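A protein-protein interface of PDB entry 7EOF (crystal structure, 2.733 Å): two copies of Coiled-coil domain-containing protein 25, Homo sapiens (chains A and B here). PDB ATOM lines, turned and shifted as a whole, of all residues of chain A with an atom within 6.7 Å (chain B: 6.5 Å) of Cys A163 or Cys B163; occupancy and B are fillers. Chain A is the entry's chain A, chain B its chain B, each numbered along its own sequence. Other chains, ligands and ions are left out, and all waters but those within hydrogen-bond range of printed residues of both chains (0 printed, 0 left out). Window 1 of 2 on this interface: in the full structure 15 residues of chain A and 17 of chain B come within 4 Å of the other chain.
N of Phe B154 sits at hydrogen-bond distance from OE2 of Glu A167. O of Phe B154 sits at hydrogen-bond distance from ND2 of Asn A170, at 2.9 Å. The side-chain carboxylate (OD2) of Asp B156 is in salt-bridge range of the guanidinium group (NH1) of Arg A166 (3.1 Å). O of Ala B159 is in hydrogen-bond range of SG of Cys A163 (3.4 Å). The side-chain sulfur of Cys A163 sits at hydrogen-bond distance from the backbone NH of Glu B160. O of Ala A159 lies close to SG of Cys B163. N of Glu A160 sits at hydrogen-bond distance from SG of Cys B163 (3.5 Å). The side-chain sulfur (SG) of Cys B163 sits at hydrogen-bond distance from the side-chain sulfur (SG) of Cys A163, 3.5 Å away. OD2 of Asp A156 is in salt-bridge range of NH1 of Arg B166 (3.2 Å). The side-chain carboxylate (OE2) of Glu B167 lies within hydrogen-bond range of the backbone NH (N) of Phe A154 (3.3 Å).
Of the 17 printed residues of chain A, 8 touch a printed residue of chain B. Hydrophobic or aromatic side chains of chain A within 4 Å of the printed part of chain B: Ala A159. Of the 16 printed residues of chain B, 9 touch a printed residue of chain A. Printed residues of chain B that touch a printed residue of chain A: Arg B153, Phe B154, Pro B155, Asp B156, Ala B159, Glu B160, Cys B163, Arg B166 and Glu B167. Hydrophobic or aromatic side chains of chain B within 4 Å of the printed part of chain A: Phe B154 and Ala B159. Among the printed residues, Asp or Glu carboxylates within 4 Å of a Lys or Arg side-chain nitrogen of the other chain: Asp A156 with Arg B166 and Arg A166 with Asp B156.
Phe A154 touches Glu B167, and with the chains exchanged Glu A167 touches Phe B154. Asp A156 touches Arg B166, and with the chains exchanged Arg A166 touches Asp B156. Cys A163 touches its own counterpart, Cys B163. Glu A167 touches Pro B155, but with the chains exchanged Pro A155 does not touch Glu B167 (4.1 Å). Positions printed for both chains: 47, 154, 155, 156, 158, 159, 160, 161, 162, 163, 164, 165, 166, 167 and 168.
Among the printed residues, merely in contact across the chains: Ala A159 with Arg B166, Arg A166 with Ala B159, Glu A167 with Arg B153, Glu A167 with Pro B155 and Asn A170 with Pro B155.
Of the printed residues of chain B, Cys A163 touches Ala B159 (3.4 Å), Glu B160 (3.6 Å) and Cys B163 (3.5 Å). Cys B163 touches just these residues of chain A: Ala A159 (3.4 Å), Glu A160 (3.5 Å) and Cys A163 (3.5 Å). Of the printed residues of chain B, Phe A154 touches Glu B167 (3.3 Å). Printed residues of chain A within 4 Å of Arg B166: Asp A156 and Ala A159. Of the printed residues of chain A, Ala B159 touches Cys A163 (3.4 Å) and Arg A166 (3.8 Å). Printed residues of chain A within 4 Å of Arg B153: Glu A167 (3.3 Å). Of the printed residues of chain B, Glu A160 touches Cys B163. The nearest residue of chain A that does not touch Cys B163 is Asp A156 (4.6 Å). The nearest printed residue of chain A that does not touch Ala B159 is Ala A159 (5.6 Å).
The side-chain carboxylate of Glu B160 is in salt-bridge range of the guanidinium group of Arg B153, at 3.2 Å. The side-chain carboxylate (OD1) of Asp B156 sits at hydrogen-bond distance from the backbone NH (N) of Ala B159 (3.2 Å). O of Ala B159 lies within hydrogen-bond range of SG of Cys B163. OD1 of Asp A156 is in hydrogen-bond range of N of Ala A159. The backbone carbonyl oxygen (O) of Ala A159 sits at hydrogen-bond distance from the side-chain sulfur (SG) of Cys A163 (3.4 Å). NE of Arg A166 lies within salt-bridge range of OE1 of Glu A162 (3.0 Å).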
ATOM      1  N   TRP A  47     -32.067   5.020 -14.990  1.00  0.00           N
ATOM      2  CA  TRP A  47     -30.963   4.380 -15.697  1.00  0.00           C
ATOM      3  C   TRP A  47     -30.372   3.238 -14.879  1.00  0.00           C
ATOM      4  O   TRP A  47     -30.455   3.239 -13.647  1.00  0.00           O
ATOM      5  CB  TRP A  47     -29.861   5.392 -16.005  1.00  0.00           C
ATOM      6  CG  TRP A  47     -30.259   6.457 -16.968  1.00  0.00           C
ATOM      7  CD1 TRP A  47     -31.514   6.710 -17.440  1.00  0.00           C
ATOM      8  CD2 TRP A  47     -29.396   7.416 -17.586  1.00  0.00           C
ATOM      9  NE1 TRP A  47     -31.487   7.773 -18.308  1.00  0.00           N
ATOM     10  CE2 TRP A  47     -30.199   8.225 -18.414  1.00  0.00           C
ATOM     11  CE3 TRP A  47     -28.026   7.673 -17.515  1.00  0.00           C
ATOM     12  CZ2 TRP A  47     -29.674   9.271 -19.168  1.00  0.00           C
ATOM     13  CZ3 TRP A  47     -27.508   8.711 -18.260  1.00  0.00           C
ATOM     14  CH2 TRP A  47     -28.329   9.497 -19.078  1.00  0.00           C
ATOM     15  N   PHE A 154     -36.456  20.339 -16.864  1.00  0.00           N
ATOM     16  CA  PHE A 154     -37.659  19.706 -17.394  1.00  0.00           C
ATOM     17  C   PHE A 154     -37.248  18.710 -18.473  1.00  0.00           C
ATOM     18  O   PHE A 154     -37.504  18.920 -19.667  1.00  0.00           O
ATOM     19  CB  PHE A 154     -38.632  20.746 -17.939  1.00  0.00           C
ATOM     20  CG  PHE A 154     -39.302  21.550 -16.872  1.00  0.00           C
ATOM     21  CD1 PHE A 154     -38.643  22.604 -16.263  1.00  0.00           C
ATOM     22  CD2 PHE A 154     -40.591  21.246 -16.469  1.00  0.00           C
ATOM     23  CE1 PHE A 154     -39.262  23.346 -15.277  1.00  0.00           C
ATOM     24  CE2 PHE A 154     -41.219  21.987 -15.486  1.00  0.00           C
ATOM     25  CZ  PHE A 154     -40.554  23.038 -14.889  1.00  0.00           C
ATOM     26  N   PRO A 155     -36.609  17.614 -18.082  1.00  0.00           N
ATOM     27  CA  PRO A 155     -36.008  16.713 -19.063  1.00  0.00           C
ATOM     28  C   PRO A 155     -37.039  15.838 -19.755  1.00  0.00           C
ATOM     29  O   PRO A 155     -38.157  15.636 -19.279  1.00  0.00           O
ATOM     30  CB  PRO A 155     -35.068  15.863 -18.208  1.00  0.00           C
ATOM     31  CG  PRO A 155     -35.793  15.764 -16.905  1.00  0.00           C
ATOM     32  CD  PRO A 155     -36.486  17.091 -16.711  1.00  0.00           C
ATOM     33  N   ASP A 156     -36.620  15.296 -20.894  1.00  0.00           N
ATOM     34  CA  ASP A 156     -37.334  14.217 -21.563  1.00  0.00           C
ATOM     35  C   ASP A 156     -36.597  12.943 -21.181  1.00  0.00           C
ATOM     36  O   ASP A 156     -35.515  12.661 -21.704  1.00  0.00           O
ATOM     37  CB  ASP A 156     -37.347  14.430 -23.075  1.00  0.00           C
ATOM     38  CG  ASP A 156     -38.194  13.409 -23.811  1.00  0.00           C
ATOM     39  OD1 ASP A 156     -38.337  12.265 -23.327  1.00  0.00           O
ATOM     40  OD2 ASP A 156     -38.713  13.756 -24.893  1.00  0.00           O
ATOM     41  N   LEU A 157     -37.197  12.160 -20.293  1.00  0.00           N
ATOM     42  CA  LEU A 157     -36.436  11.090 -19.666  1.00  0.00           C
ATOM     43  C   LEU A 157     -36.299   9.886 -20.585  1.00  0.00           C
ATOM     44  O   LEU A 157     -35.240   9.249 -20.619  1.00  0.00           O
ATOM     45  CB  LEU A 157     -37.084  10.701 -18.342  1.00  0.00           C
ATOM     46  CG  LEU A 157     -37.049  11.813 -17.290  1.00  0.00           C
ATOM     47  CD1 LEU A 157     -38.293  12.690 -17.363  1.00  0.00           C
ATOM     48  CD2 LEU A 157     -36.888  11.221 -15.912  1.00  0.00           C
ATOM     49  N   ALA A 158     -37.350   9.567 -21.341  1.00  0.00           N
ATOM     50  CA  ALA A 158     -37.267   8.466 -22.294  1.00  0.00           C
ATOM     51  C   ALA A 158     -36.216   8.742 -23.361  1.00  0.00           C
ATOM     52  O   ALA A 158     -35.458   7.843 -23.749  1.00  0.00           O
ATOM     53  CB  ALA A 158     -38.632   8.225 -22.935  1.00  0.00           C
ATOM     54  N   ALA A 159     -36.150   9.982 -23.846  1.00  0.00           N
ATOM     55  CA  ALA A 159     -35.149  10.326 -24.848  1.00  0.00           C
ATOM     56  C   ALA A 159     -33.744  10.293 -24.260  1.00  0.00           C
ATOM     57  O   ALA A 159     -32.788   9.895 -24.938  1.00  0.00           O
ATOM     58  CB  ALA A 159     -35.457  11.699 -25.442  1.00  0.00           C
ATOM     59  N   GLU A 160     -33.596  10.703 -23.000  1.00  0.00           N
ATOM     60  CA  GLU A 160     -32.277  10.706 -22.379  1.00  0.00           C
ATOM     61  C   GLU A 160     -31.776   9.288 -22.135  1.00  0.00           C
ATOM     62  O   GLU A 160     -30.623   8.961 -22.452  1.00  0.00           O
ATOM     63  CB  GLU A 160     -32.314  11.508 -21.080  1.00  0.00           C
ATOM     64  CG  GLU A 160     -32.308  13.003 -21.314  1.00  0.00           C
ATOM     65  CD  GLU A 160     -32.106  13.784 -20.039  1.00  0.00           C
ATOM     66  OE1 GLU A 160     -32.251  15.025 -20.076  1.00  0.00           O
ATOM     67  OE2 GLU A 160     -31.804  13.154 -19.003  1.00  0.00           O
ATOM     68  N   LYS A 161     -32.629   8.425 -21.575  1.00  0.00           N
ATOM     69  CA  LYS A 161     -32.241   7.027 -21.434  1.00  0.00           C
ATOM     70  C   LYS A 161     -31.991   6.386 -22.791  1.00  0.00           C
ATOM     71  O   LYS A 161     -31.130   5.506 -22.913  1.00  0.00           O
ATOM     72  CB  LYS A 161     -33.306   6.245 -20.664  1.00  0.00           C
ATOM     73  CG  LYS A 161     -32.835   4.858 -20.259  1.00  0.00           C
ATOM     74  CD  LYS A 161     -33.934   4.046 -19.620  1.00  0.00           C
ATOM     75  CE  LYS A 161     -33.444   2.643 -19.304  1.00  0.00           C
ATOM     76  NZ  LYS A 161     -34.533   1.774 -18.783  1.00  0.00           N
ATOM     77  N   GLU A 162     -32.721   6.823 -23.823  1.00  0.00           N
ATOM     78  CA  GLU A 162     -32.440   6.351 -25.174  1.00  0.00           C
ATOM     79  C   GLU A 162     -31.038   6.755 -25.613  1.00  0.00           C
ATOM     80  O   GLU A 162     -30.328   5.964 -26.241  1.00  0.00           O
ATOM     81  CB  GLU A 162     -33.487   6.886 -26.150  1.00  0.00           C
ATOM     82  CG  GLU A 162     -33.246   6.501 -27.605  1.00  0.00           C
ATOM     83  CD  GLU A 162     -33.236   4.998 -27.826  1.00  0.00           C
ATOM     84  OE1 GLU A 162     -32.374   4.509 -28.587  1.00  0.00           O
ATOM     85  OE2 GLU A 162     -34.092   4.305 -27.237  1.00  0.00           O
ATOM     86  N   CYS A 163     -30.622   7.983 -25.291  1.00  0.00           N
ATOM     87  CA  CYS A 163     -29.253   8.398 -25.582  1.00  0.00           C
ATOM     88  C   CYS A 163     -28.250   7.507 -24.864  1.00  0.00           C
ATOM     89  O   CYS A 163     -27.277   7.037 -25.466  1.00  0.00           O
ATOM     90  CB  CYS A 163     -29.044   9.858 -25.186  1.00  0.00           C
ATOM     91  SG  CYS A 163     -29.854  11.047 -26.262  1.00  0.00           S
ATOM     92  N   ARG A 164     -28.471   7.268 -23.570  1.00  0.00           N
ATOM     93  CA  ARG A 164     -27.563   6.409 -22.817  1.00  0.00           C
ATOM     94  C   ARG A 164     -27.448   5.032 -23.464  1.00  0.00           C
ATOM     95  O   ARG A 164     -26.343   4.502 -23.645  1.00  0.00           O
ATOM     96  CB  ARG A 164     -28.043   6.286 -21.374  1.00  0.00           C
ATOM     97  CG  ARG A 164     -27.212   5.339 -20.549  1.00  0.00           C
ATOM     98  CD  ARG A 164     -28.087   4.455 -19.696  1.00  0.00           C
ATOM     99  NE  ARG A 164     -27.331   3.335 -19.150  1.00  0.00           N
ATOM    100  CZ  ARG A 164     -27.099   2.203 -19.807  1.00  0.00           C
ATOM    101  NH1 ARG A 164     -26.400   1.237 -19.231  1.00  0.00           N
ATOM    102  NH2 ARG A 164     -27.564   2.040 -21.038  1.00  0.00           N
ATOM    103  N   ASP A 165     -28.587   4.450 -23.842  1.00  0.00           N
ATOM    104  CA  ASP A 165     -28.579   3.130 -24.460  1.00  0.00           C
ATOM    105  C   ASP A 165     -27.907   3.148 -25.827  1.00  0.00           C
ATOM    106  O   ASP A 165     -27.254   2.169 -26.204  1.00  0.00           O
ATOM    107  CB  ASP A 165     -30.006   2.600 -24.569  1.00  0.00           C
ATOM    108  CG  ASP A 165     -30.669   2.443 -23.214  1.00  0.00           C
ATOM    109  OD1 ASP A 165     -29.954   2.155 -22.231  1.00  0.00           O
ATOM    110  OD2 ASP A 165     -31.902   2.611 -23.131  1.00  0.00           O
ATOM    111  N   ARG A 166     -28.053   4.236 -26.584  1.00  0.00           N
ATOM    112  CA  ARG A 166     -27.342   4.340 -27.851  1.00  0.00           C
ATOM    113  C   ARG A 166     -25.838   4.394 -27.629  1.00  0.00           C
ATOM    114  O   ARG A 166     -25.072   3.783 -28.383  1.00  0.00           O
ATOM    115  CB  ARG A 166     -27.819   5.566 -28.628  1.00  0.00           C
ATOM    116  CG  ARG A 166     -29.240   5.439 -29.136  1.00  0.00           C
ATOM    117  CD  ARG A 166     -29.634   6.605 -30.021  1.00  0.00           C
ATOM    118  NE  ARG A 166     -31.032   6.501 -30.428  1.00  0.00           N
ATOM    119  CZ  ARG A 166     -31.612   7.294 -31.321  1.00  0.00           C
ATOM    120  NH1 ARG A 166     -30.910   8.253 -31.909  1.00  0.00           N
ATOM    121  NH2 ARG A 166     -32.890   7.127 -31.630  1.00  0.00           N
ATOM    122  N   GLU A 167     -25.399   5.115 -26.594  1.00  0.00           N
ATOM    123  CA  GLU A 167     -23.980   5.130 -26.253  1.00  0.00           C
ATOM    124  C   GLU A 167     -23.490   3.730 -25.912  1.00  0.00           C
ATOM    125  O   GLU A 167     -22.414   3.312 -26.361  1.00  0.00           O
ATOM    126  CB  GLU A 167     -23.735   6.087 -25.087  1.00  0.00           C
ATOM    127  CG  GLU A 167     -22.299   6.588 -24.962  1.00  0.00           C
ATOM    128  CD  GLU A 167     -21.351   5.549 -24.392  1.00  0.00           C
ATOM    129  OE1 GLU A 167     -21.809   4.651 -23.656  1.00  0.00           O
ATOM    130  OE2 GLU A 167     -20.142   5.630 -24.683  1.00  0.00           O
ATOM    131  N   GLU A 168     -24.266   2.992 -25.115  1.00  0.00           N
ATOM    132  CA  GLU A 168     -23.889   1.619 -24.789  1.00  0.00           C
ATOM    133  C   GLU A 168     -23.797   0.759 -26.043  1.00  0.00           C
ATOM    134  O   GLU A 168     -22.846  -0.014 -26.212  1.00  0.00           O
ATOM    135  CB  GLU A 168     -24.898   1.030 -23.807  1.00  0.00           C
ATOM    136  CG  GLU A 168     -24.409  -0.185 -23.052  1.00  0.00           C
ATOM    137  CD  GLU A 168     -25.448  -0.704 -22.079  1.00  0.00           C
ATOM    138  OE1 GLU A 168     -26.645  -0.714 -22.439  1.00  0.00           O
ATOM    139  OE2 GLU A 168     -25.072  -1.087 -20.952  1.00  0.00           O
ATOM    140  N   ASN A 170     -23.217   1.722 -29.212  1.00  0.00           N
ATOM    141  CA  ASN A 170     -22.031   2.092 -29.976  1.00  0.00           C
ATOM    142  C   ASN A 170     -20.770   1.540 -29.331  1.00  0.00           C
ATOM    143  O   ASN A 170     -19.854   1.076 -30.027  1.00  0.00           O
ATOM    144  CB  ASN A 170     -21.933   3.612 -30.101  1.00  0.00           C
ATOM    145  CG  ASN A 170     -23.151   4.226 -30.745  1.00  0.00           C
ATOM    146  OD1 ASN A 170     -23.920   3.547 -31.423  1.00  0.00           O
ATOM    147  ND2 ASN A 170     -23.332   5.524 -30.542  1.00  0.00           N
ATOM    148  N   TRP B  47     -23.525  22.359 -28.516  1.00  0.00           N
ATOM    149  CA  TRP B  47     -24.605  23.039 -27.814  1.00  0.00           C
ATOM    150  C   TRP B  47     -24.329  24.531 -27.695  1.00  0.00           C
ATOM    151  O   TRP B  47     -23.178  24.970 -27.756  1.00  0.00           O
ATOM    152  CB  TRP B  47     -24.783  22.447 -26.419  1.00  0.00           C
ATOM    153  CG  TRP B  47     -25.197  21.015 -26.391  1.00  0.00           C
ATOM    154  CD1 TRP B  47     -25.243  20.152 -27.442  1.00  0.00           C
ATOM    155  CD2 TRP B  47     -25.630  20.277 -25.246  1.00  0.00           C
ATOM    156  NE1 TRP B  47     -25.674  18.918 -27.023  1.00  0.00           N
ATOM    157  CE2 TRP B  47     -25.918  18.968 -25.676  1.00  0.00           C
ATOM    158  CE3 TRP B  47     -25.803  20.595 -23.896  1.00  0.00           C
ATOM    159  CZ2 TRP B  47     -26.371  17.981 -24.809  1.00  0.00           C
ATOM    160  CZ3 TRP B  47     -26.251  19.613 -23.036  1.00  0.00           C
ATOM    161  CH2 TRP B  47     -26.529  18.324 -23.495  1.00  0.00           C
ATOM    162  N   ARG B 153     -16.128   7.902 -24.495  1.00  0.00           N
ATOM    163  CA  ARG B 153     -17.534   7.665 -24.776  1.00  0.00           C
ATOM    164  C   ARG B 153     -17.751   7.524 -26.276  1.00  0.00           C
ATOM    165  O   ARG B 153     -16.926   7.944 -27.090  1.00  0.00           O
ATOM    166  CB  ARG B 153     -18.418   8.783 -24.212  1.00  0.00           C
ATOM    167  CG  ARG B 153     -19.275   8.367 -23.026  1.00  0.00           C
ATOM    168  CD  ARG B 153     -20.502   9.268 -22.912  1.00  0.00           C
ATOM    169  NE  ARG B 153     -21.474   8.775 -21.939  1.00  0.00           N
ATOM    170  CZ  ARG B 153     -22.731   9.207 -21.855  1.00  0.00           C
ATOM    171  NH1 ARG B 153     -23.172  10.139 -22.691  1.00  0.00           N
ATOM    172  NH2 ARG B 153     -23.549   8.703 -20.939  1.00  0.00           N
ATOM    173  N   PHE B 154     -18.881   6.912 -26.628  1.00  0.00           N
ATOM    174  CA  PHE B 154     -19.311   6.742 -28.013  1.00  0.00           C
ATOM    175  C   PHE B 154     -20.716   7.312 -28.151  1.00  0.00           C
ATOM    176  O   PHE B 154     -21.678   6.582 -28.421  1.00  0.00           O
ATOM    177  CB  PHE B 154     -19.271   5.275 -28.432  1.00  0.00           C
ATOM    178  CG  PHE B 154     -17.890   4.765 -28.701  1.00  0.00           C
ATOM    179  CD1 PHE B 154     -17.067   4.374 -27.660  1.00  0.00           C
ATOM    180  CD2 PHE B 154     -17.412   4.682 -29.997  1.00  0.00           C
ATOM    181  CE1 PHE B 154     -15.795   3.909 -27.905  1.00  0.00           C
ATOM    182  CE2 PHE B 154     -16.142   4.216 -30.251  1.00  0.00           C
ATOM    183  CZ  PHE B 154     -15.330   3.829 -29.202  1.00  0.00           C
ATOM    184  N   PRO B 155     -20.865   8.619 -27.977  1.00  0.00           N
ATOM    185  CA  PRO B 155     -22.198   9.208 -27.874  1.00  0.00           C
ATOM    186  C   PRO B 155     -22.882   9.332 -29.224  1.00  0.00           C
ATOM    187  O   PRO B 155     -22.261   9.256 -30.285  1.00  0.00           O
ATOM    188  CB  PRO B 155     -21.928  10.595 -27.278  1.00  0.00           C
ATOM    189  CG  PRO B 155     -20.405  10.784 -27.319  1.00  0.00           C
ATOM    190  CD  PRO B 155     -19.829   9.652 -28.105  1.00  0.00           C
ATOM    191  N   ASP B 156     -24.193   9.532 -29.160  1.00  0.00           N
ATOM    192  CA  ASP B 156     -24.970   9.978 -30.306  1.00  0.00           C
ATOM    193  C   ASP B 156     -25.180  11.473 -30.109  1.00  0.00           C
ATOM    194  O   ASP B 156     -26.018  11.890 -29.301  1.00  0.00           O
ATOM    195  CB  ASP B 156     -26.296   9.224 -30.383  1.00  0.00           C
ATOM    196  CG  ASP B 156     -27.079   9.532 -31.648  1.00  0.00           C
ATOM    197  OD1 ASP B 156     -26.901  10.628 -32.223  1.00  0.00           O
ATOM    198  OD2 ASP B 156     -27.887   8.672 -32.064  1.00  0.00           O
ATOM    199  N   ALA B 158     -26.259  14.075 -32.118  1.00  0.00           N
ATOM    200  CA  ALA B 158     -27.540  14.647 -32.509  1.00  0.00           C
ATOM    201  C   ALA B 158     -28.638  14.279 -31.522  1.00  0.00           C
ATOM    202  O   ALA B 158     -29.520  15.096 -31.244  1.00  0.00           O
ATOM    203  CB  ALA B 158     -27.915  14.186 -33.918  1.00  0.00           C
ATOM    204  N   ALA B 159     -28.602  13.058 -30.986  1.00  0.00           N
ATOM    205  CA  ALA B 159     -29.621  12.645 -30.029  1.00  0.00           C
ATOM    206  C   ALA B 159     -29.476  13.395 -28.714  1.00  0.00           C
ATOM    207  O   ALA B 159     -30.472  13.833 -28.129  1.00  0.00           O
ATOM    208  CB  ALA B 159     -29.545  11.137 -29.806  1.00  0.00           C
ATOM    209  N   GLU B 160     -28.244  13.552 -28.230  1.00  0.00           N
ATOM    210  CA  GLU B 160     -28.049  14.238 -26.959  1.00  0.00           C
ATOM    211  C   GLU B 160     -28.398  15.717 -27.070  1.00  0.00           C
ATOM    212  O   GLU B 160     -29.010  16.289 -26.158  1.00  0.00           O
ATOM    213  CB  GLU B 160     -26.614  14.039 -26.480  1.00  0.00           C
ATOM    214  CG  GLU B 160     -26.309  12.594 -26.145  1.00  0.00           C
ATOM    215  CD  GLU B 160     -24.956  12.425 -25.498  1.00  0.00           C
ATOM    216  OE1 GLU B 160     -24.507  11.268 -25.344  1.00  0.00           O
ATOM    217  OE2 GLU B 160     -24.341  13.452 -25.144  1.00  0.00           O
ATOM    218  N   LYS B 161     -28.041  16.351 -28.190  1.00  0.00           N
ATOM    219  CA  LYS B 161     -28.488  17.723 -28.399  1.00  0.00           C
ATOM    220  C   LYS B 161     -29.997  17.790 -28.568  1.00  0.00           C
ATOM    221  O   LYS B 161     -30.624  18.770 -28.152  1.00  0.00           O
ATOM    222  CB  LYS B 161     -27.794  18.344 -29.607  1.00  0.00           C
ATOM    223  CG  LYS B 161     -28.125  19.815 -29.784  1.00  0.00           C
ATOM    224  CD  LYS B 161     -27.357  20.418 -30.931  1.00  0.00           C
ATOM    225  CE  LYS B 161     -27.627  21.902 -31.056  1.00  0.00           C
ATOM    226  NZ  LYS B 161     -26.751  22.500 -32.099  1.00  0.00           N
ATOM    227  N   GLU B 162     -30.597  16.765 -29.172  1.00  0.00           N
ATOM    228  CA  GLU B 162     -32.051  16.705 -29.242  1.00  0.00           C
ATOM    229  C   GLU B 162     -32.659  16.706 -27.847  1.00  0.00           C
ATOM    230  O   GLU B 162     -33.638  17.416 -27.589  1.00  0.00           O
ATOM    231  CB  GLU B 162     -32.490  15.470 -30.028  1.00  0.00           C
ATOM    232  CG  GLU B 162     -33.990  15.199 -29.997  1.00  0.00           C
ATOM    233  CD  GLU B 162     -34.805  16.250 -30.735  1.00  0.00           C
ATOM    234  OE1 GLU B 162     -34.224  17.001 -31.547  1.00  0.00           O
ATOM    235  OE2 GLU B 162     -36.031  16.321 -30.503  1.00  0.00           O
ATOM    236  N   CYS B 163     -32.081  15.930 -26.925  1.00  0.00           N
ATOM    237  CA  CYS B 163     -32.548  15.958 -25.543  1.00  0.00           C
ATOM    238  C   CYS B 163     -32.400  17.347 -24.938  1.00  0.00           C
ATOM    239  O   CYS B 163     -33.322  17.848 -24.284  1.00  0.00           O
ATOM    240  CB  CYS B 163     -31.791  14.932 -24.705  1.00  0.00           C
ATOM    241  SG  CYS B 163     -32.305  13.235 -24.993  1.00  0.00           S
ATOM    242  N   ARG B 164     -31.246  17.985 -25.152  1.00  0.00           N
ATOM    243  CA  ARG B 164     -31.047  19.341 -24.646  1.00  0.00           C
ATOM    244  C   ARG B 164     -32.131  20.291 -25.151  1.00  0.00           C
ATOM    245  O   ARG B 164     -32.742  21.036 -24.369  1.00  0.00           O
ATOM    246  CB  ARG B 164     -29.664  19.842 -25.053  1.00  0.00           C
ATOM    247  CG  ARG B 164     -29.403  21.268 -24.655  1.00  0.00           C
ATOM    248  CD  ARG B 164     -28.716  22.035 -25.760  1.00  0.00           C
ATOM    249  NE  ARG B 164     -28.694  23.460 -25.457  1.00  0.00           N
ATOM    250  CZ  ARG B 164     -29.670  24.304 -25.775  1.00  0.00           C
ATOM    251  NH1 ARG B 164     -29.572  25.583 -25.451  1.00  0.00           N
ATOM    252  NH2 ARG B 164     -30.742  23.868 -26.420  1.00  0.00           N
ATOM    253  N   ASP B 165     -32.388  20.272 -26.460  1.00  0.00           N
ATOM    254  CA  ASP B 165     -33.380  21.170 -27.041  1.00  0.00           C
ATOM    255  C   ASP B 165     -34.776  20.860 -26.524  1.00  0.00           C
ATOM    256  O   ASP B 165     -35.581  21.773 -26.303  1.00  0.00           O
ATOM    257  CB  ASP B 165     -33.341  21.079 -28.563  1.00  0.00           C
ATOM    258  CG  ASP B 165     -32.055  21.629 -29.144  1.00  0.00           C
ATOM    259  OD1 ASP B 165     -31.351  22.366 -28.422  1.00  0.00           O
ATOM    260  OD2 ASP B 165     -31.752  21.332 -30.320  1.00  0.00           O
ATOM    261  N   ARG B 166     -35.085  19.581 -26.320  1.00  0.00           N
ATOM    262  CA  ARG B 166     -36.380  19.239 -25.749  1.00  0.00           C
ATOM    263  C   ARG B 166     -36.516  19.774 -24.329  1.00  0.00           C
ATOM    264  O   ARG B 166     -37.587  20.258 -23.948  1.00  0.00           O
ATOM    265  CB  ARG B 166     -36.592  17.729 -25.786  1.00  0.00           C
ATOM    266  CG  ARG B 166     -36.841  17.212 -27.181  1.00  0.00           C
ATOM    267  CD  ARG B 166     -37.132  15.731 -27.179  1.00  0.00           C
ATOM    268  NE  ARG B 166     -37.199  15.211 -28.539  1.00  0.00           N
ATOM    269  CZ  ARG B 166     -37.536  13.965 -28.842  1.00  0.00           C
ATOM    270  NH1 ARG B 166     -37.840  13.112 -27.874  1.00  0.00           N
ATOM    271  NH2 ARG B 166     -37.570  13.572 -30.108  1.00  0.00           N
ATOM    272  N   GLU B 167     -35.443  19.712 -23.533  1.00  0.00           N
ATOM    273  CA  GLU B 167     -35.508  20.296 -22.197  1.00  0.00           C
ATOM    274  C   GLU B 167     -35.758  21.796 -22.270  1.00  0.00           C
ATOM    275  O   GLU B 167     -36.578  22.330 -21.514  1.00  0.00           O
ATOM    276  CB  GLU B 167     -34.227  20.010 -21.415  1.00  0.00           C
ATOM    277  CG  GLU B 167     -34.299  20.400 -19.929  1.00  0.00           C
ATOM    278  CD  GLU B 167     -34.076  21.887 -19.679  1.00  0.00           C
ATOM    279  OE1 GLU B 167     -33.376  22.530 -20.489  1.00  0.00           O
ATOM    280  OE2 GLU B 167     -34.604  22.418 -18.679  1.00  0.00           O
ATOM    281  N   GLU B 168     -35.056  22.495 -23.165  1.00  0.00           N
ATOM    282  CA  GLU B 168     -35.294  23.929 -23.302  1.00  0.00           C
ATOM    283  C   GLU B 168     -36.739  24.215 -23.697  1.00  0.00           C
ATOM    284  O   GLU B 168     -37.373  25.133 -23.158  1.00  0.00           O
ATOM    285  CB  GLU B 168     -34.330  24.523 -24.322  1.00  0.00           C
ATOM    286  CG  GLU B 168     -34.661  25.945 -24.707  1.00  0.00           C
ATOM    287  CD  GLU B 168     -33.585  26.572 -25.554  1.00  0.00           C
ATOM    288  OE1 GLU B 168     -32.624  27.120 -24.977  1.00  0.00           O
ATOM    289  OE2 GLU B 168     -33.693  26.502 -26.796  1.00  0.00           O
